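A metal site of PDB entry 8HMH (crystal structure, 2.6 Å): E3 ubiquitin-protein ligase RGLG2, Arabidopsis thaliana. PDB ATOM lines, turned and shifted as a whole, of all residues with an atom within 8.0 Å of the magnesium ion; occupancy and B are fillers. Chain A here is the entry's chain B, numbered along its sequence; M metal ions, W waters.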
ATOM      1  N   ASP A  55      16.324  13.387 -25.442  1.00  0.00           N
ATOM      2  CA  ASP A  55      16.587  14.812 -25.375  1.00  0.00           C
ATOM      3  C   ASP A  55      16.931  15.402 -26.752  1.00  0.00           C
ATOM      4  O   ASP A  55      17.959  15.056 -27.354  1.00  0.00           O
ATOM      5  CB  ASP A  55      17.739  15.019 -24.384  1.00  0.00           C
ATOM      6  CG  ASP A  55      18.088  16.468 -24.141  1.00  0.00           C
ATOM      7  OD1 ASP A  55      17.981  17.312 -25.064  1.00  0.00           O
ATOM      8  OD2 ASP A  55      18.501  16.756 -23.002  1.00  0.00           O
ATOM      9  N   PHE A  56      16.093  16.316 -27.232  1.00  0.00           N
ATOM     10  CA  PHE A  56      16.431  16.971 -28.484  1.00  0.00           C
ATOM     11  C   PHE A  56      16.664  18.493 -28.268  1.00  0.00           C
ATOM     12  O   PHE A  56      16.235  19.305 -29.077  1.00  0.00           O
ATOM     13  CB  PHE A  56      15.352  16.704 -29.537  1.00  0.00           C
ATOM     14  CG  PHE A  56      15.305  15.258 -30.016  1.00  0.00           C
ATOM     15  CD1 PHE A  56      16.364  14.710 -30.735  1.00  0.00           C
ATOM     16  CD2 PHE A  56      14.192  14.449 -29.726  1.00  0.00           C
ATOM     17  CE1 PHE A  56      16.321  13.372 -31.160  1.00  0.00           C
ATOM     18  CE2 PHE A  56      14.151  13.121 -30.150  1.00  0.00           C
ATOM     19  CZ  PHE A  56      15.214  12.583 -30.878  1.00  0.00           C
ATOM     20  N   THR A  57      17.374  18.865 -27.200  1.00  0.00           N
ATOM     21  CA  THR A  57      17.640  20.277 -26.953  1.00  0.00           C
ATOM     22  C   THR A  57      18.784  20.765 -27.857  1.00  0.00           C
ATOM     23  O   THR A  57      19.587  19.962 -28.347  1.00  0.00           O
ATOM     24  CB  THR A  57      17.951  20.549 -25.448  1.00  0.00           C
ATOM     25  OG1 THR A  57      19.164  19.887 -25.012  1.00  0.00           O
ATOM     26  CG2 THR A  57      16.766  20.102 -24.590  1.00  0.00           C
ATOM     27  N   LYS A  58      18.824  22.079 -28.128  1.00  0.00           N
ATOM     28  CA  LYS A  58      19.820  22.655 -29.048  1.00  0.00           C
ATOM     29  C   LYS A  58      21.271  22.585 -28.518  1.00  0.00           C
ATOM     30  O   LYS A  58      22.210  22.694 -29.292  1.00  0.00           O
ATOM     31  CB  LYS A  58      19.451  24.108 -29.390  1.00  0.00           C
ATOM     32  CG  LYS A  58      19.455  25.005 -28.202  1.00  0.00           C
ATOM     33  CD  LYS A  58      19.104  26.434 -28.548  1.00  0.00           C
ATOM     34  CE  LYS A  58      17.625  26.669 -28.728  1.00  0.00           C
ATOM     35  NZ  LYS A  58      17.394  28.141 -28.824  1.00  0.00           N
ATOM     36  N   SER A  59      21.430  22.429 -27.204  1.00  0.00           N
ATOM     37  CA  SER A  59      22.747  22.233 -26.571  1.00  0.00           C
ATOM     38  C   SER A  59      23.497  20.985 -27.103  1.00  0.00           C
ATOM     39  O   SER A  59      24.727  20.869 -26.972  1.00  0.00           O
ATOM     40  CB  SER A  59      22.597  22.098 -25.053  1.00  0.00           C
ATOM     41  OG  SER A  59      21.751  20.984 -24.719  1.00  0.00           O
ATOM     42  N   ASN A  60      22.770  20.034 -27.687  1.00  0.00           N
ATOM     43  CA  ASN A  60      23.389  18.808 -28.198  1.00  0.00           C
ATOM     44  C   ASN A  60      24.424  19.114 -29.308  1.00  0.00           C
ATOM     45  O   ASN A  60      25.249  18.261 -29.696  1.00  0.00           O
ATOM     46  CB  ASN A  60      22.313  17.822 -28.719  1.00  0.00           C
ATOM     47  CG  ASN A  60      21.600  17.090 -27.580  1.00  0.00           C
ATOM     48  OD1 ASN A  60      22.189  16.209 -26.940  1.00  0.00           O
ATOM     49  ND2 ASN A  60      20.344  17.439 -27.328  1.00  0.00           N
ATOM     50  N   GLU A  61      24.388  20.336 -29.826  1.00  0.00           N
ATOM     51  CA  GLU A  61      25.366  20.709 -30.848  1.00  0.00           C
ATOM     52  C   GLU A  61      26.762  20.870 -30.271  1.00  0.00           C
ATOM     53  O   GLU A  61      27.743  20.607 -30.940  1.00  0.00           O
ATOM     54  CB  GLU A  61      24.947  21.990 -31.534  1.00  0.00           C
ATOM     55  CG  GLU A  61      23.820  21.777 -32.507  1.00  0.00           C
ATOM     56  CD  GLU A  61      24.198  20.933 -33.685  1.00  0.00           C
ATOM     57  OE1 GLU A  61      25.429  20.675 -33.871  1.00  0.00           O
ATOM     58  OE2 GLU A  61      23.255  20.507 -34.399  1.00  0.00           O
ATOM     59  N   TRP A  62      26.844  21.259 -29.009  1.00  0.00           N
ATOM     60  CA  TRP A  62      28.146  21.580 -28.441  1.00  0.00           C
ATOM     61  C   TRP A  62      28.560  20.695 -27.269  1.00  0.00           C
ATOM     62  O   TRP A  62      29.722  20.705 -26.855  1.00  0.00           O
ATOM     63  CB  TRP A  62      28.182  23.040 -27.986  1.00  0.00           C
ATOM     64  CG  TRP A  62      27.299  23.393 -26.810  1.00  0.00           C
ATOM     65  CD1 TRP A  62      27.515  23.084 -25.499  1.00  0.00           C
ATOM     66  CD2 TRP A  62      26.111  24.207 -26.837  1.00  0.00           C
ATOM     67  NE1 TRP A  62      26.508  23.628 -24.710  1.00  0.00           N
ATOM     68  CE2 TRP A  62      25.644  24.324 -25.505  1.00  0.00           C
ATOM     69  CE3 TRP A  62      25.382  24.833 -27.862  1.00  0.00           C
ATOM     70  CZ2 TRP A  62      24.490  25.046 -25.174  1.00  0.00           C
ATOM     71  CZ3 TRP A  62      24.234  25.544 -27.518  1.00  0.00           C
ATOM     72  CH2 TRP A  62      23.796  25.645 -26.188  1.00  0.00           C
ATOM     73  N   THR A  63      27.609  19.972 -26.704  1.00  0.00           N
ATOM     74  CA  THR A  63      27.912  19.168 -25.537  1.00  0.00           C
ATOM     75  C   THR A  63      28.742  17.948 -25.936  1.00  0.00           C
ATOM     76  O   THR A  63      29.161  17.165 -25.078  1.00  0.00           O
ATOM     77  CB  THR A  63      26.632  18.739 -24.835  1.00  0.00           C
ATOM     78  OG1 THR A  63      25.733  18.107 -25.779  1.00  0.00           O
ATOM     79  CG2 THR A  63      25.990  19.972 -24.215  1.00  0.00           C
ATOM     80  N   LEU A  73      25.883  15.616 -30.498  1.00  0.00           N
ATOM     81  CA  LEU A  73      25.496  14.361 -29.888  1.00  0.00           C
ATOM     82  C   LEU A  73      24.477  13.645 -30.777  1.00  0.00           C
ATOM     83  O   LEU A  73      24.407  12.417 -30.789  1.00  0.00           O
ATOM     84  CB  LEU A  73      24.957  14.608 -28.484  1.00  0.00           C
ATOM     85  CG  LEU A  73      25.999  14.973 -27.422  1.00  0.00           C
ATOM     86  CD1 LEU A  73      25.361  14.903 -26.043  1.00  0.00           C
ATOM     87  CD2 LEU A  73      27.233  14.054 -27.465  1.00  0.00           C
ATOM     88  N   TYR A  83      23.563   8.758 -27.864  1.00  0.00           N
ATOM     89  CA  TYR A  83      22.183   8.408 -27.626  1.00  0.00           C
ATOM     90  C   TYR A  83      21.982   6.980 -28.115  1.00  0.00           C
ATOM     91  O   TYR A  83      21.426   6.135 -27.389  1.00  0.00           O
ATOM     92  CB  TYR A  83      21.197   9.372 -28.312  1.00  0.00           C
ATOM     93  CG  TYR A  83      21.066  10.713 -27.618  1.00  0.00           C
ATOM     94  CD1 TYR A  83      21.924  11.782 -27.916  1.00  0.00           C
ATOM     95  CD2 TYR A  83      20.112  10.908 -26.614  1.00  0.00           C
ATOM     96  CE1 TYR A  83      21.806  13.001 -27.271  1.00  0.00           C
ATOM     97  CE2 TYR A  83      20.002  12.116 -25.967  1.00  0.00           C
ATOM     98  CZ  TYR A  83      20.845  13.159 -26.302  1.00  0.00           C
ATOM     99  OH  TYR A  83      20.721  14.359 -25.649  1.00  0.00           O
ATOM    100  N   ALA A 148      15.612  22.496 -29.773  1.00  0.00           N
ATOM    101  CA  ALA A 148      15.138  23.693 -29.066  1.00  0.00           C
ATOM    102  C   ALA A 148      15.447  23.630 -27.565  1.00  0.00           C
ATOM    103  O   ALA A 148      16.536  23.227 -27.178  1.00  0.00           O
ATOM    104  CB  ALA A 148      13.648  23.852 -29.293  1.00  0.00           C
ATOM    105  N   GLY A 149      14.481  24.021 -26.732  1.00  0.00           N
ATOM    106  CA  GLY A 149      14.691  24.112 -25.293  1.00  0.00           C
ATOM    107  C   GLY A 149      13.515  24.795 -24.622  1.00  0.00           C
ATOM    108  O   GLY A 149      12.519  25.120 -25.306  1.00  0.00           O
ATOM    109  N   PRO A 150      13.583  25.010 -23.293  1.00  0.00           N
ATOM    110  CA  PRO A 150      14.669  24.615 -22.401  1.00  0.00           C
ATOM    111  C   PRO A 150      14.441  23.179 -21.930  1.00  0.00           C
ATOM    112  O   PRO A 150      13.695  22.449 -22.582  1.00  0.00           O
ATOM    113  CB  PRO A 150      14.558  25.627 -21.250  1.00  0.00           C
ATOM    114  CG  PRO A 150      13.087  25.892 -21.143  1.00  0.00           C
ATOM    115  CD  PRO A 150      12.504  25.693 -22.558  1.00  0.00           C
ATOM    116  N   THR A 151      15.083  22.768 -20.837  1.00  0.00           N
ATOM    117  CA  THR A 151      15.076  21.367 -20.429  1.00  0.00           C
ATOM    118  C   THR A 151      14.255  21.084 -19.176  1.00  0.00           C
ATOM    119  O   THR A 151      14.521  21.616 -18.094  1.00  0.00           O
ATOM    120  CB  THR A 151      16.519  20.873 -20.232  1.00  0.00           C
ATOM    121  OG1 THR A 151      17.241  21.081 -21.456  1.00  0.00           O
ATOM    122  CG2 THR A 151      16.543  19.409 -19.857  1.00  0.00           C
ATOM    123  N   PHE A 153      12.139  17.477 -17.438  1.00  0.00           N
ATOM    124  CA  PHE A 153      11.830  16.065 -17.583  1.00  0.00           C
ATOM    125  C   PHE A 153      10.419  15.798 -17.134  1.00  0.00           C
ATOM    126  O   PHE A 153       9.961  14.649 -17.157  1.00  0.00           O
ATOM    127  CB  PHE A 153      12.827  15.215 -16.798  1.00  0.00           C
ATOM    128  CG  PHE A 153      14.226  15.413 -17.251  1.00  0.00           C
ATOM    129  CD1 PHE A 153      14.516  15.391 -18.609  1.00  0.00           C
ATOM    130  CD2 PHE A 153      15.238  15.672 -16.358  1.00  0.00           C
ATOM    131  CE1 PHE A 153      15.792  15.580 -19.051  1.00  0.00           C
ATOM    132  CE2 PHE A 153      16.514  15.881 -16.789  1.00  0.00           C
ATOM    133  CZ  PHE A 153      16.796  15.829 -18.139  1.00  0.00           C
ATOM    134  N   ALA A 178      19.513  12.278 -21.599  1.00  0.00           N
ATOM    135  CA  ALA A 178      19.623  13.726 -21.773  1.00  0.00           C
ATOM    136  C   ALA A 178      21.072  14.231 -21.765  1.00  0.00           C
ATOM    137  O   ALA A 178      21.963  13.578 -21.224  1.00  0.00           O
ATOM    138  CB  ALA A 178      18.811  14.461 -20.708  1.00  0.00           C
ATOM    139  N   ASP A 179      21.279  15.414 -22.361  1.00  0.00           N
ATOM    140  CA  ASP A 179      22.622  16.005 -22.440  1.00  0.00           C
ATOM    141  C   ASP A 179      22.839  17.131 -21.433  1.00  0.00           C
ATOM    142  O   ASP A 179      23.928  17.708 -21.396  1.00  0.00           O
ATOM    143  CB  ASP A 179      22.948  16.509 -23.845  1.00  0.00           C
ATOM    144  CG  ASP A 179      22.409  17.906 -24.127  1.00  0.00           C
ATOM    145  OD1 ASP A 179      21.357  18.280 -23.565  1.00  0.00           O
ATOM    146  OD2 ASP A 179      23.058  18.637 -24.908  1.00  0.00           O
ATOM    147  N   GLY A 180      21.805  17.467 -20.655  1.00  0.00           N
ATOM    148  CA  GLY A 180      21.972  18.402 -19.550  1.00  0.00           C
ATOM    149  C   GLY A 180      20.957  18.354 -18.411  1.00  0.00           C
ATOM    150  O   GLY A 180      19.917  17.712 -18.538  1.00  0.00           O
ATOM    151  N   GLN A 181      21.250  19.021 -17.298  1.00  0.00           N
ATOM    152  CA  GLN A 181      20.322  19.009 -16.172  1.00  0.00           C
ATOM    153  C   GLN A 181      19.152  19.927 -16.424  1.00  0.00           C
ATOM    154  O   GLN A 181      19.201  20.724 -17.360  1.00  0.00           O
ATOM    155  CB  GLN A 181      21.000  19.371 -14.851  1.00  0.00           C
ATOM    156  CG  GLN A 181      22.033  20.454 -14.923  1.00  0.00           C
ATOM    157  CD  GLN A 181      23.169  20.245 -13.908  1.00  0.00           C
ATOM    158  OE1 GLN A 181      23.289  19.185 -13.288  1.00  0.00           O
ATOM    159  NE2 GLN A 181      23.999  21.278 -13.753  1.00  0.00           N
ATOM    160  N   VAL A 182      18.098  19.805 -15.603  1.00  0.00           N
ATOM    161  CA  VAL A 182      16.907  20.649 -15.768  1.00  0.00           C
ATOM    162  C   VAL A 182      17.256  22.146 -15.788  1.00  0.00           C
ATOM    163  O   VAL A 182      18.014  22.626 -14.934  1.00  0.00           O
ATOM    164  CB  VAL A 182      15.874  20.413 -14.657  1.00  0.00           C
ATOM    165  CG1 VAL A 182      14.685  21.251 -14.895  1.00  0.00           C
ATOM    166  CG2 VAL A 182      15.481  18.974 -14.630  1.00  0.00           C
ATOM    167  N   THR A 183      16.676  22.863 -16.753  1.00  0.00           N
ATOM    168  CA  THR A 183      16.955  24.281 -16.934  1.00  0.00           C
ATOM    169  C   THR A 183      16.696  25.087 -15.654  1.00  0.00           C
ATOM    170  O   THR A 183      15.612  25.007 -15.075  1.00  0.00           O
ATOM    171  CB  THR A 183      16.110  24.904 -18.060  1.00  0.00           C
ATOM    172  OG1 THR A 183      16.461  24.315 -19.328  1.00  0.00           O
ATOM    173  CG2 THR A 183      16.351  26.411 -18.105  1.00  0.00           C
ATOM    174  N   VAL A 219      24.281  11.931 -21.032  1.00  0.00           N
ATOM    175  CA  VAL A 219      25.284  11.833 -22.092  1.00  0.00           C
ATOM    176  C   VAL A 219      25.892  13.213 -22.418  1.00  0.00           C
ATOM    177  O   VAL A 219      25.338  14.254 -22.055  1.00  0.00           O
ATOM    178  CB  VAL A 219      24.705  11.175 -23.341  1.00  0.00           C
ATOM    179  CG1 VAL A 219      24.279   9.731 -22.987  1.00  0.00           C
ATOM    180  CG2 VAL A 219      23.528  11.960 -23.880  1.00  0.00           C
ATOM    181  N   GLY A 222      27.906  17.664 -20.360  1.00  0.00           N
ATOM    182  CA  GLY A 222      27.157  18.095 -19.182  1.00  0.00           C
ATOM    183  C   GLY A 222      27.037  19.603 -19.041  1.00  0.00           C
ATOM    184  O   GLY A 222      26.629  20.309 -19.980  1.00  0.00           O
ATOM    185  N   TRP A 224      27.533  17.616 -15.134  1.00  0.00           N
ATOM    186  CA  TRP A 224      26.730  16.716 -14.311  1.00  0.00           C
ATOM    187  C   TRP A 224      27.180  16.816 -12.878  1.00  0.00           C
ATOM    188  O   TRP A 224      27.002  15.879 -12.091  1.00  0.00           O
ATOM    189  CB  TRP A 224      26.834  15.264 -14.794  1.00  0.00           C
ATOM    190  CG  TRP A 224      26.460  15.140 -16.213  1.00  0.00           C
ATOM    191  CD1 TRP A 224      27.280  14.933 -17.271  1.00  0.00           C
ATOM    192  CD2 TRP A 224      25.137  15.259 -16.743  1.00  0.00           C
ATOM    193  NE1 TRP A 224      26.559  14.884 -18.436  1.00  0.00           N
ATOM    194  CE2 TRP A 224      25.242  15.099 -18.142  1.00  0.00           C
ATOM    195  CE3 TRP A 224      23.880  15.475 -16.176  1.00  0.00           C
ATOM    196  CZ2 TRP A 224      24.125  15.151 -18.983  1.00  0.00           C
ATOM    197  CZ3 TRP A 224      22.778  15.523 -17.002  1.00  0.00           C
ATOM    198  CH2 TRP A 224      22.904  15.369 -18.394  1.00  0.00           C
HETATM  199 MG    MG M   1      20.821  20.298 -23.084  1.00  0.00          MG
HETATM  200  O   HOH W   1      19.036  19.382 -22.447  1.00  0.00           O
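The backbone carbonyl oxygen (O) of Ser 59 lies close to the side-chain hydroxyl (OG1) of Thr 63 (3.2 Å).
N of Asp 179 is in hydrogen-bond range of OD2 of Asp 55, at 3.2 Å.
OD2 of Asp 179 is in hydrogen-bond range of N of Asn 60 (3.1 Å).
The side-chain carboxylate (OD2) of Asp 179 is in hydrogen-bond range of the side-chain hydroxyl (OG1) of Thr 63.
The side-chain hydroxyl (OH) of Tyr 83 is in hydrogen-bond range of the backbone NH (N) of Asp 179 (3.5 Å).
OD1 of Asp 55 sits at hydrogen-bond distance from N of Thr 57, 2.7 Å away.
The side-chain amide nitrogen of Asn 60 lies within hydrogen-bond range of the backbone carbonyl oxygen of Thr 57.
Merely in contact with the magnesium ion: Gly 180.
Within 4 Å of the magnesium ion: Thr 57, Ser 59, Asp 179 and Gly 180.
The magnesium ion is bound by OG of Ser 59 (2.0 Å), water W1 (2.1 Å), OD1 of Asp 179 (2.1 Å) and OG1 of Thr 57 (2.6 Å).
The magnesium ion has four donor atoms within binding distance.
Water W1 bridges the side-chain hydroxyl of Thr 151 and the side-chain carboxylate of Asp 55.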
